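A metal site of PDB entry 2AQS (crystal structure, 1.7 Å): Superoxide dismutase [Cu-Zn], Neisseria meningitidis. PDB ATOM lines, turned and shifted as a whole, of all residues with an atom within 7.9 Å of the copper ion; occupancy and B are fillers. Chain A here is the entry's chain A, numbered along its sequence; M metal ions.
NE2 of His 59 binds the copper ion (2.0 Å).
The copper ion is bound by a ring nitrogen (NE2) of His 138.
The copper ion is bound by ND1 of His 57.
The copper ion has three donor atoms within binding distance.
O of Gly 81 sits close to ND1 of His 59 (3.3 Å).
ND1 of His 59 lies within hydrogen-bond range of O of Gly 80, at 2.9 Å.
The backbone NH (N) of His 59 sits at hydrogen-bond distance from the backbone carbonyl oxygen (O) of Ser 134, at 2.8 Å.
A ring nitrogen (ND1) of His 138 sits at hydrogen-bond distance from the backbone carbonyl oxygen (O) of Gly 155 (3.0 Å).
A ring nitrogen (ND1) of His 138 sits at hydrogen-bond distance from the backbone carbonyl oxygen (O) of Pro 156 (3.2 Å).
ND1 of His 57 sits close to NE2 of His 82, 3.3 Å away.
The backbone carbonyl oxygen of His 57 sits at hydrogen-bond distance from the backbone NH of Met 136 (2.7 Å).
A ring nitrogen (NE2) of His 57 sits at hydrogen-bond distance from the side-chain carboxylate (OD2) of Asp 142 (2.9 Å).
His 82 touches the copper ion.
Met 136 touches the copper ion (CB to CU, 3.8 Å).
Of the 25 residues printed, 5 come within 4 Å of the copper ion.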
ATOM      1  N   GLY A  55      -6.419  -7.938 -33.400  1.00  0.00           N
ATOM      2  CA  GLY A  55      -7.778  -8.152 -32.940  1.00  0.00           C
ATOM      3  C   GLY A  55      -8.305  -6.828 -32.415  1.00  0.00           C
ATOM      4  O   GLY A  55      -7.589  -6.107 -31.721  1.00  0.00           O
ATOM      5  N   PHE A  56      -9.557  -6.531 -32.724  1.00  0.00           N
ATOM      6  CA  PHE A  56     -10.160  -5.267 -32.342  1.00  0.00           C
ATOM      7  C   PHE A  56     -11.577  -5.564 -31.855  1.00  0.00           C
ATOM      8  O   PHE A  56     -12.414  -5.997 -32.627  1.00  0.00           O
ATOM      9  CB  PHE A  56     -10.147  -4.387 -33.603  1.00  0.00           C
ATOM     10  CG  PHE A  56     -10.584  -2.971 -33.390  1.00  0.00           C
ATOM     11  CD1 PHE A  56     -10.091  -2.228 -32.327  1.00  0.00           C
ATOM     12  CD2 PHE A  56     -11.414  -2.353 -34.322  1.00  0.00           C
ATOM     13  CE1 PHE A  56     -10.421  -0.890 -32.194  1.00  0.00           C
ATOM     14  CE2 PHE A  56     -11.746  -1.017 -34.207  1.00  0.00           C
ATOM     15  CZ  PHE A  56     -11.252  -0.282 -33.149  1.00  0.00           C
ATOM     16  N   HIS A  57     -11.827  -5.369 -30.557  1.00  0.00           N
ATOM     17  CA  HIS A  57     -13.149  -5.643 -29.998  1.00  0.00           C
ATOM     18  C   HIS A  57     -13.596  -4.695 -28.898  1.00  0.00           C
ATOM     19  O   HIS A  57     -12.783  -4.037 -28.238  1.00  0.00           O
ATOM     20  CB  HIS A  57     -13.233  -7.051 -29.392  1.00  0.00           C
ATOM     21  CG  HIS A  57     -12.246  -8.030 -29.962  1.00  0.00           C
ATOM     22  ND1 HIS A  57     -11.123  -8.431 -29.275  1.00  0.00           N
ATOM     23  CD2 HIS A  57     -12.248  -8.721 -31.131  1.00  0.00           C
ATOM     24  CE1 HIS A  57     -10.461  -9.313 -29.996  1.00  0.00           C
ATOM     25  NE2 HIS A  57     -11.121  -9.514 -31.131  1.00  0.00           N
ATOM     26  N   ILE A  58     -14.905  -4.627 -28.698  1.00  0.00           N
ATOM     27  CA  ILE A  58     -15.473  -3.825 -27.634  1.00  0.00           C
ATOM     28  C   ILE A  58     -15.516  -4.784 -26.439  1.00  0.00           C
ATOM     29  O   ILE A  58     -15.983  -5.920 -26.561  1.00  0.00           O
ATOM     30  CB  ILE A  58     -16.923  -3.371 -27.960  1.00  0.00           C
ATOM     31  CG1 ILE A  58     -16.919  -2.528 -29.241  1.00  0.00           C
ATOM     32  CG2 ILE A  58     -17.510  -2.624 -26.779  1.00  0.00           C
ATOM     33  CD1 ILE A  58     -16.180  -1.228 -29.159  1.00  0.00           C
ATOM     34  N   HIS A  59     -15.010  -4.341 -25.298  1.00  0.00           N
ATOM     35  CA  HIS A  59     -15.017  -5.163 -24.106  1.00  0.00           C
ATOM     36  C   HIS A  59     -16.063  -4.627 -23.140  1.00  0.00           C
ATOM     37  O   HIS A  59     -16.416  -3.452 -23.186  1.00  0.00           O
ATOM     38  CB  HIS A  59     -13.617  -5.232 -23.477  1.00  0.00           C
ATOM     39  CG  HIS A  59     -12.692  -6.171 -24.192  1.00  0.00           C
ATOM     40  ND1 HIS A  59     -12.105  -7.257 -23.578  1.00  0.00           N
ATOM     41  CD2 HIS A  59     -12.291  -6.219 -25.488  1.00  0.00           C
ATOM     42  CE1 HIS A  59     -11.383  -7.930 -24.463  1.00  0.00           C
ATOM     43  NE2 HIS A  59     -11.487  -7.316 -25.630  1.00  0.00           N
ATOM     44  N   ALA A  79     -10.849  -4.383 -18.280  1.00  0.00           N
ATOM     45  CA  ALA A  79     -11.872  -4.205 -19.288  1.00  0.00           C
ATOM     46  C   ALA A  79     -12.853  -5.373 -19.321  1.00  0.00           C
ATOM     47  O   ALA A  79     -13.936  -5.269 -19.894  1.00  0.00           O
ATOM     48  CB  ALA A  79     -11.229  -4.038 -20.652  1.00  0.00           C
ATOM     49  N   GLY A  80     -12.480  -6.491 -18.715  1.00  0.00           N
ATOM     50  CA  GLY A  80     -13.364  -7.649 -18.727  1.00  0.00           C
ATOM     51  C   GLY A  80     -13.252  -8.378 -20.057  1.00  0.00           C
ATOM     52  O   GLY A  80     -12.289  -8.171 -20.798  1.00  0.00           O
ATOM     53  N   GLY A  81     -14.238  -9.218 -20.357  1.00  0.00           N
ATOM     54  CA  GLY A  81     -14.201  -9.974 -21.603  1.00  0.00           C
ATOM     55  C   GLY A  81     -14.845  -9.248 -22.780  1.00  0.00           C
ATOM     56  O   GLY A  81     -15.191  -8.066 -22.688  1.00  0.00           O
ATOM     57  N   HIS A  82     -14.977  -9.945 -23.906  1.00  0.00           N
ATOM     58  CA  HIS A  82     -15.599  -9.344 -25.073  1.00  0.00           C
ATOM     59  C   HIS A  82     -17.031  -8.975 -24.729  1.00  0.00           C
ATOM     60  O   HIS A  82     -17.739  -9.757 -24.092  1.00  0.00           O
ATOM     61  CB  HIS A  82     -15.605 -10.325 -26.256  1.00  0.00           C
ATOM     62  CG  HIS A  82     -14.251 -10.605 -26.823  1.00  0.00           C
ATOM     63  ND1 HIS A  82     -14.078 -11.172 -28.061  1.00  0.00           N
ATOM     64  CD2 HIS A  82     -13.010 -10.409 -26.317  1.00  0.00           C
ATOM     65  CE1 HIS A  82     -12.788 -11.321 -28.305  1.00  0.00           C
ATOM     66  NE2 HIS A  82     -12.109 -10.868 -27.260  1.00  0.00           N
ATOM     67  N   TRP A  83     -17.447  -7.786 -25.141  1.00  0.00           N
ATOM     68  CA  TRP A  83     -18.810  -7.329 -24.884  1.00  0.00           C
ATOM     69  C   TRP A  83     -19.774  -8.284 -25.612  1.00  0.00           C
ATOM     70  O   TRP A  83     -19.748  -8.401 -26.831  1.00  0.00           O
ATOM     71  CB  TRP A  83     -18.979  -5.908 -25.407  1.00  0.00           C
ATOM     72  CG  TRP A  83     -20.287  -5.294 -25.052  1.00  0.00           C
ATOM     73  CD1 TRP A  83     -20.918  -5.334 -23.845  1.00  0.00           C
ATOM     74  CD2 TRP A  83     -21.114  -4.497 -25.909  1.00  0.00           C
ATOM     75  NE1 TRP A  83     -22.081  -4.609 -23.893  1.00  0.00           N
ATOM     76  CE2 TRP A  83     -22.231  -4.089 -25.146  1.00  0.00           C
ATOM     77  CE3 TRP A  83     -21.011  -4.085 -27.245  1.00  0.00           C
ATOM     78  CZ2 TRP A  83     -23.248  -3.285 -25.677  1.00  0.00           C
ATOM     79  CZ3 TRP A  83     -22.028  -3.282 -27.776  1.00  0.00           C
ATOM     80  CH2 TRP A  83     -23.128  -2.899 -26.991  1.00  0.00           C
ATOM     81  N   HIS A  91     -16.959 -16.286 -29.912  1.00  0.00           N
ATOM     82  CA  HIS A  91     -16.301 -15.270 -30.716  1.00  0.00           C
ATOM     83  C   HIS A  91     -16.509 -15.554 -32.199  1.00  0.00           C
ATOM     84  O   HIS A  91     -16.435 -16.712 -32.633  1.00  0.00           O
ATOM     85  CB  HIS A  91     -14.808 -15.224 -30.395  1.00  0.00           C
ATOM     86  CG  HIS A  91     -14.069 -14.159 -31.133  1.00  0.00           C
ATOM     87  ND1 HIS A  91     -14.236 -12.817 -30.849  1.00  0.00           N
ATOM     88  CD2 HIS A  91     -13.194 -14.224 -32.152  1.00  0.00           C
ATOM     89  CE1 HIS A  91     -13.487 -12.100 -31.676  1.00  0.00           C
ATOM     90  NE2 HIS A  91     -12.840 -12.934 -32.474  1.00  0.00           N
ATOM     91  N   GLY A 102     -19.530  -7.343 -29.567  1.00  0.00           N
ATOM     92  CA  GLY A 102     -18.340  -6.510 -29.554  1.00  0.00           C
ATOM     93  C   GLY A 102     -17.262  -6.909 -30.540  1.00  0.00           C
ATOM     94  O   GLY A 102     -16.203  -6.279 -30.569  1.00  0.00           O
ATOM     95  N   ASP A 103     -17.519  -7.922 -31.368  1.00  0.00           N
ATOM     96  CA  ASP A 103     -16.526  -8.382 -32.331  1.00  0.00           C
ATOM     97  C   ASP A 103     -16.451  -7.487 -33.550  1.00  0.00           C
ATOM     98  O   ASP A 103     -17.335  -7.507 -34.413  1.00  0.00           O
ATOM     99  CB  ASP A 103     -16.818  -9.827 -32.739  1.00  0.00           C
ATOM    100  CG  ASP A 103     -16.646 -10.789 -31.575  1.00  0.00           C
ATOM    101  OD1 ASP A 103     -16.028 -10.389 -30.571  1.00  0.00           O
ATOM    102  OD2 ASP A 103     -17.125 -11.947 -31.665  1.00  0.00           O
ATOM    103  N   SER A 134     -15.367  -0.450 -23.330  1.00  0.00           N
ATOM    104  CA  SER A 134     -14.006  -0.159 -23.761  1.00  0.00           C
ATOM    105  C   SER A 134     -13.728  -0.764 -25.124  1.00  0.00           C
ATOM    106  O   SER A 134     -14.434  -1.655 -25.573  1.00  0.00           O
ATOM    107  CB  SER A 134     -12.996  -0.703 -22.744  1.00  0.00           C
ATOM    108  OG  SER A 134     -13.215  -2.070 -22.466  1.00  0.00           O
ATOM    109  N   ILE A 135     -12.706  -0.231 -25.785  1.00  0.00           N
ATOM    110  CA  ILE A 135     -12.322  -0.743 -27.087  1.00  0.00           C
ATOM    111  C   ILE A 135     -10.906  -1.285 -26.907  1.00  0.00           C
ATOM    112  O   ILE A 135     -10.037  -0.618 -26.344  1.00  0.00           O
ATOM    113  CB  ILE A 135     -12.419   0.369 -28.173  1.00  0.00           C
ATOM    114  CG1 ILE A 135     -12.242  -0.231 -29.561  1.00  0.00           C
ATOM    115  CG2 ILE A 135     -11.418   1.483 -27.905  1.00  0.00           C
ATOM    116  CD1 ILE A 135     -12.821   0.643 -30.641  1.00  0.00           C
ATOM    117  N   MET A 136     -10.690  -2.514 -27.376  1.00  0.00           N
ATOM    118  CA  MET A 136      -9.414  -3.183 -27.190  1.00  0.00           C
ATOM    119  C   MET A 136      -8.709  -3.539 -28.474  1.00  0.00           C
ATOM    120  O   MET A 136      -9.344  -3.967 -29.440  1.00  0.00           O
ATOM    121  CB  MET A 136      -9.654  -4.460 -26.371  1.00  0.00           C
ATOM    122  CG  MET A 136      -8.410  -5.074 -25.723  1.00  0.00           C
ATOM    123  SD  MET A 136      -7.833  -4.095 -24.325  1.00  0.00           S
ATOM    124  CE  MET A 136      -9.167  -4.411 -23.130  1.00  0.00           C
ATOM    125  N   ILE A 137      -7.394  -3.365 -28.493  1.00  0.00           N
ATOM    126  CA  ILE A 137      -6.570  -3.727 -29.637  1.00  0.00           C
ATOM    127  C   ILE A 137      -5.587  -4.755 -29.079  1.00  0.00           C
ATOM    128  O   ILE A 137      -4.854  -4.485 -28.129  1.00  0.00           O
ATOM    129  CB  ILE A 137      -5.784  -2.515 -30.204  1.00  0.00           C
ATOM    130  CG1 ILE A 137      -6.754  -1.408 -30.622  1.00  0.00           C
ATOM    131  CG2 ILE A 137      -4.970  -2.978 -31.415  1.00  0.00           C
ATOM    132  CD1 ILE A 137      -6.067  -0.122 -31.063  1.00  0.00           C
ATOM    133  N   HIS A 138      -5.603  -5.947 -29.662  1.00  0.00           N
ATOM    134  CA  HIS A 138      -4.760  -7.047 -29.202  1.00  0.00           C
ATOM    135  C   HIS A 138      -3.419  -7.189 -29.893  1.00  0.00           C
ATOM    136  O   HIS A 138      -3.190  -6.670 -30.986  1.00  0.00           O
ATOM    137  CB  HIS A 138      -5.535  -8.357 -29.331  1.00  0.00           C
ATOM    138  CG  HIS A 138      -6.732  -8.444 -28.429  1.00  0.00           C
ATOM    139  ND1 HIS A 138      -6.700  -9.097 -27.214  1.00  0.00           N
ATOM    140  CD2 HIS A 138      -7.966  -7.913 -28.541  1.00  0.00           C
ATOM    141  CE1 HIS A 138      -7.885  -8.969 -26.621  1.00  0.00           C
ATOM    142  NE2 HIS A 138      -8.667  -8.252 -27.403  1.00  0.00           N
ATOM    143  N   ASP A 142      -7.023 -11.749 -35.495  1.00  0.00           N
ATOM    144  CA  ASP A 142      -8.373 -12.210 -35.223  1.00  0.00           C
ATOM    145  C   ASP A 142      -8.891 -13.026 -36.401  1.00  0.00           C
ATOM    146  O   ASP A 142      -9.142 -12.476 -37.478  1.00  0.00           O
ATOM    147  CB  ASP A 142      -9.286 -10.988 -34.997  1.00  0.00           C
ATOM    148  CG  ASP A 142     -10.636 -11.367 -34.392  1.00  0.00           C
ATOM    149  OD1 ASP A 142     -11.018 -12.552 -34.459  1.00  0.00           O
ATOM    150  OD2 ASP A 142     -11.314 -10.458 -33.863  1.00  0.00           O
ATOM    151  N   LEU A 151     -11.043 -16.707 -28.667  1.00  0.00           N
ATOM    152  CA  LEU A 151     -11.178 -15.305 -29.006  1.00  0.00           C
ATOM    153  C   LEU A 151     -10.383 -14.826 -30.232  1.00  0.00           C
ATOM    154  O   LEU A 151      -9.798 -13.739 -30.217  1.00  0.00           O
ATOM    155  CB  LEU A 151     -10.812 -14.459 -27.773  1.00  0.00           C
ATOM    156  CG  LEU A 151     -11.590 -14.895 -26.517  1.00  0.00           C
ATOM    157  CD1 LEU A 151     -10.992 -14.251 -25.263  1.00  0.00           C
ATOM    158  CD2 LEU A 151     -13.055 -14.514 -26.678  1.00  0.00           C
ATOM    159  N   GLY A 154      -6.405 -13.380 -30.508  1.00  0.00           N
ATOM    160  CA  GLY A 154      -5.959 -12.049 -30.156  1.00  0.00           C
ATOM    161  C   GLY A 154      -4.924 -12.032 -29.040  1.00  0.00           C
ATOM    162  O   GLY A 154      -4.006 -11.206 -29.045  1.00  0.00           O
ATOM    163  N   GLY A 155      -5.076 -12.941 -28.090  1.00  0.00           N
ATOM    164  CA  GLY A 155      -4.121 -13.005 -26.992  1.00  0.00           C
ATOM    165  C   GLY A 155      -4.081 -11.772 -26.117  1.00  0.00           C
ATOM    166  O   GLY A 155      -5.132 -11.210 -25.785  1.00  0.00           O
ATOM    167  N   PRO A 156      -2.882 -11.309 -25.735  1.00  0.00           N
ATOM    168  CA  PRO A 156      -2.688 -10.125 -24.885  1.00  0.00           C
ATOM    169  C   PRO A 156      -3.317  -8.836 -25.396  1.00  0.00           C
ATOM    170  O   PRO A 156      -3.545  -8.650 -26.592  1.00  0.00           O
ATOM    171  CB  PRO A 156      -1.167 -10.010 -24.796  1.00  0.00           C
ATOM    172  CG  PRO A 156      -0.726 -11.440 -24.915  1.00  0.00           C
ATOM    173  CD  PRO A 156      -1.587 -11.929 -26.047  1.00  0.00           C
ATOM    174  N   ARG A 157      -3.555  -7.927 -24.458  1.00  0.00           N
ATOM    175  CA  ARG A 157      -4.152  -6.641 -24.774  1.00  0.00           C
ATOM    176  C   ARG A 157      -3.020  -5.644 -24.986  1.00  0.00           C
ATOM    177  O   ARG A 157      -2.258  -5.327 -24.067  1.00  0.00           O
ATOM    178  CB  ARG A 157      -5.101  -6.258 -23.649  1.00  0.00           C
ATOM    179  CG  ARG A 157      -6.158  -7.353 -23.512  1.00  0.00           C
ATOM    180  CD  ARG A 157      -7.095  -7.249 -22.322  1.00  0.00           C
ATOM    181  NE  ARG A 157      -7.961  -8.423 -22.289  1.00  0.00           N
ATOM    182  CZ  ARG A 157      -9.093  -8.532 -21.600  1.00  0.00           C
ATOM    183  NH1 ARG A 157      -9.533  -7.516 -20.862  1.00  0.00           N
ATOM    184  NH2 ARG A 157      -9.817  -9.644 -21.692  1.00  0.00           N
ATOM    185  N   ALA A 159      -3.389  -2.332 -26.761  1.00  0.00           N
ATOM    186  CA  ALA A 159      -3.804  -0.940 -26.579  1.00  0.00           C
ATOM    187  C   ALA A 159      -5.271  -0.943 -26.188  1.00  0.00           C
ATOM    188  O   ALA A 159      -6.008  -1.869 -26.513  1.00  0.00           O
ATOM    189  CB  ALA A 159      -3.599  -0.153 -27.868  1.00  0.00           C
HETATM  190 CU    CU M   1     -10.652  -7.967 -27.323  1.00  0.00          CU
HETATM  191 ZN    ZN M   2     -15.461 -11.845 -29.408  1.00  0.00          ZN
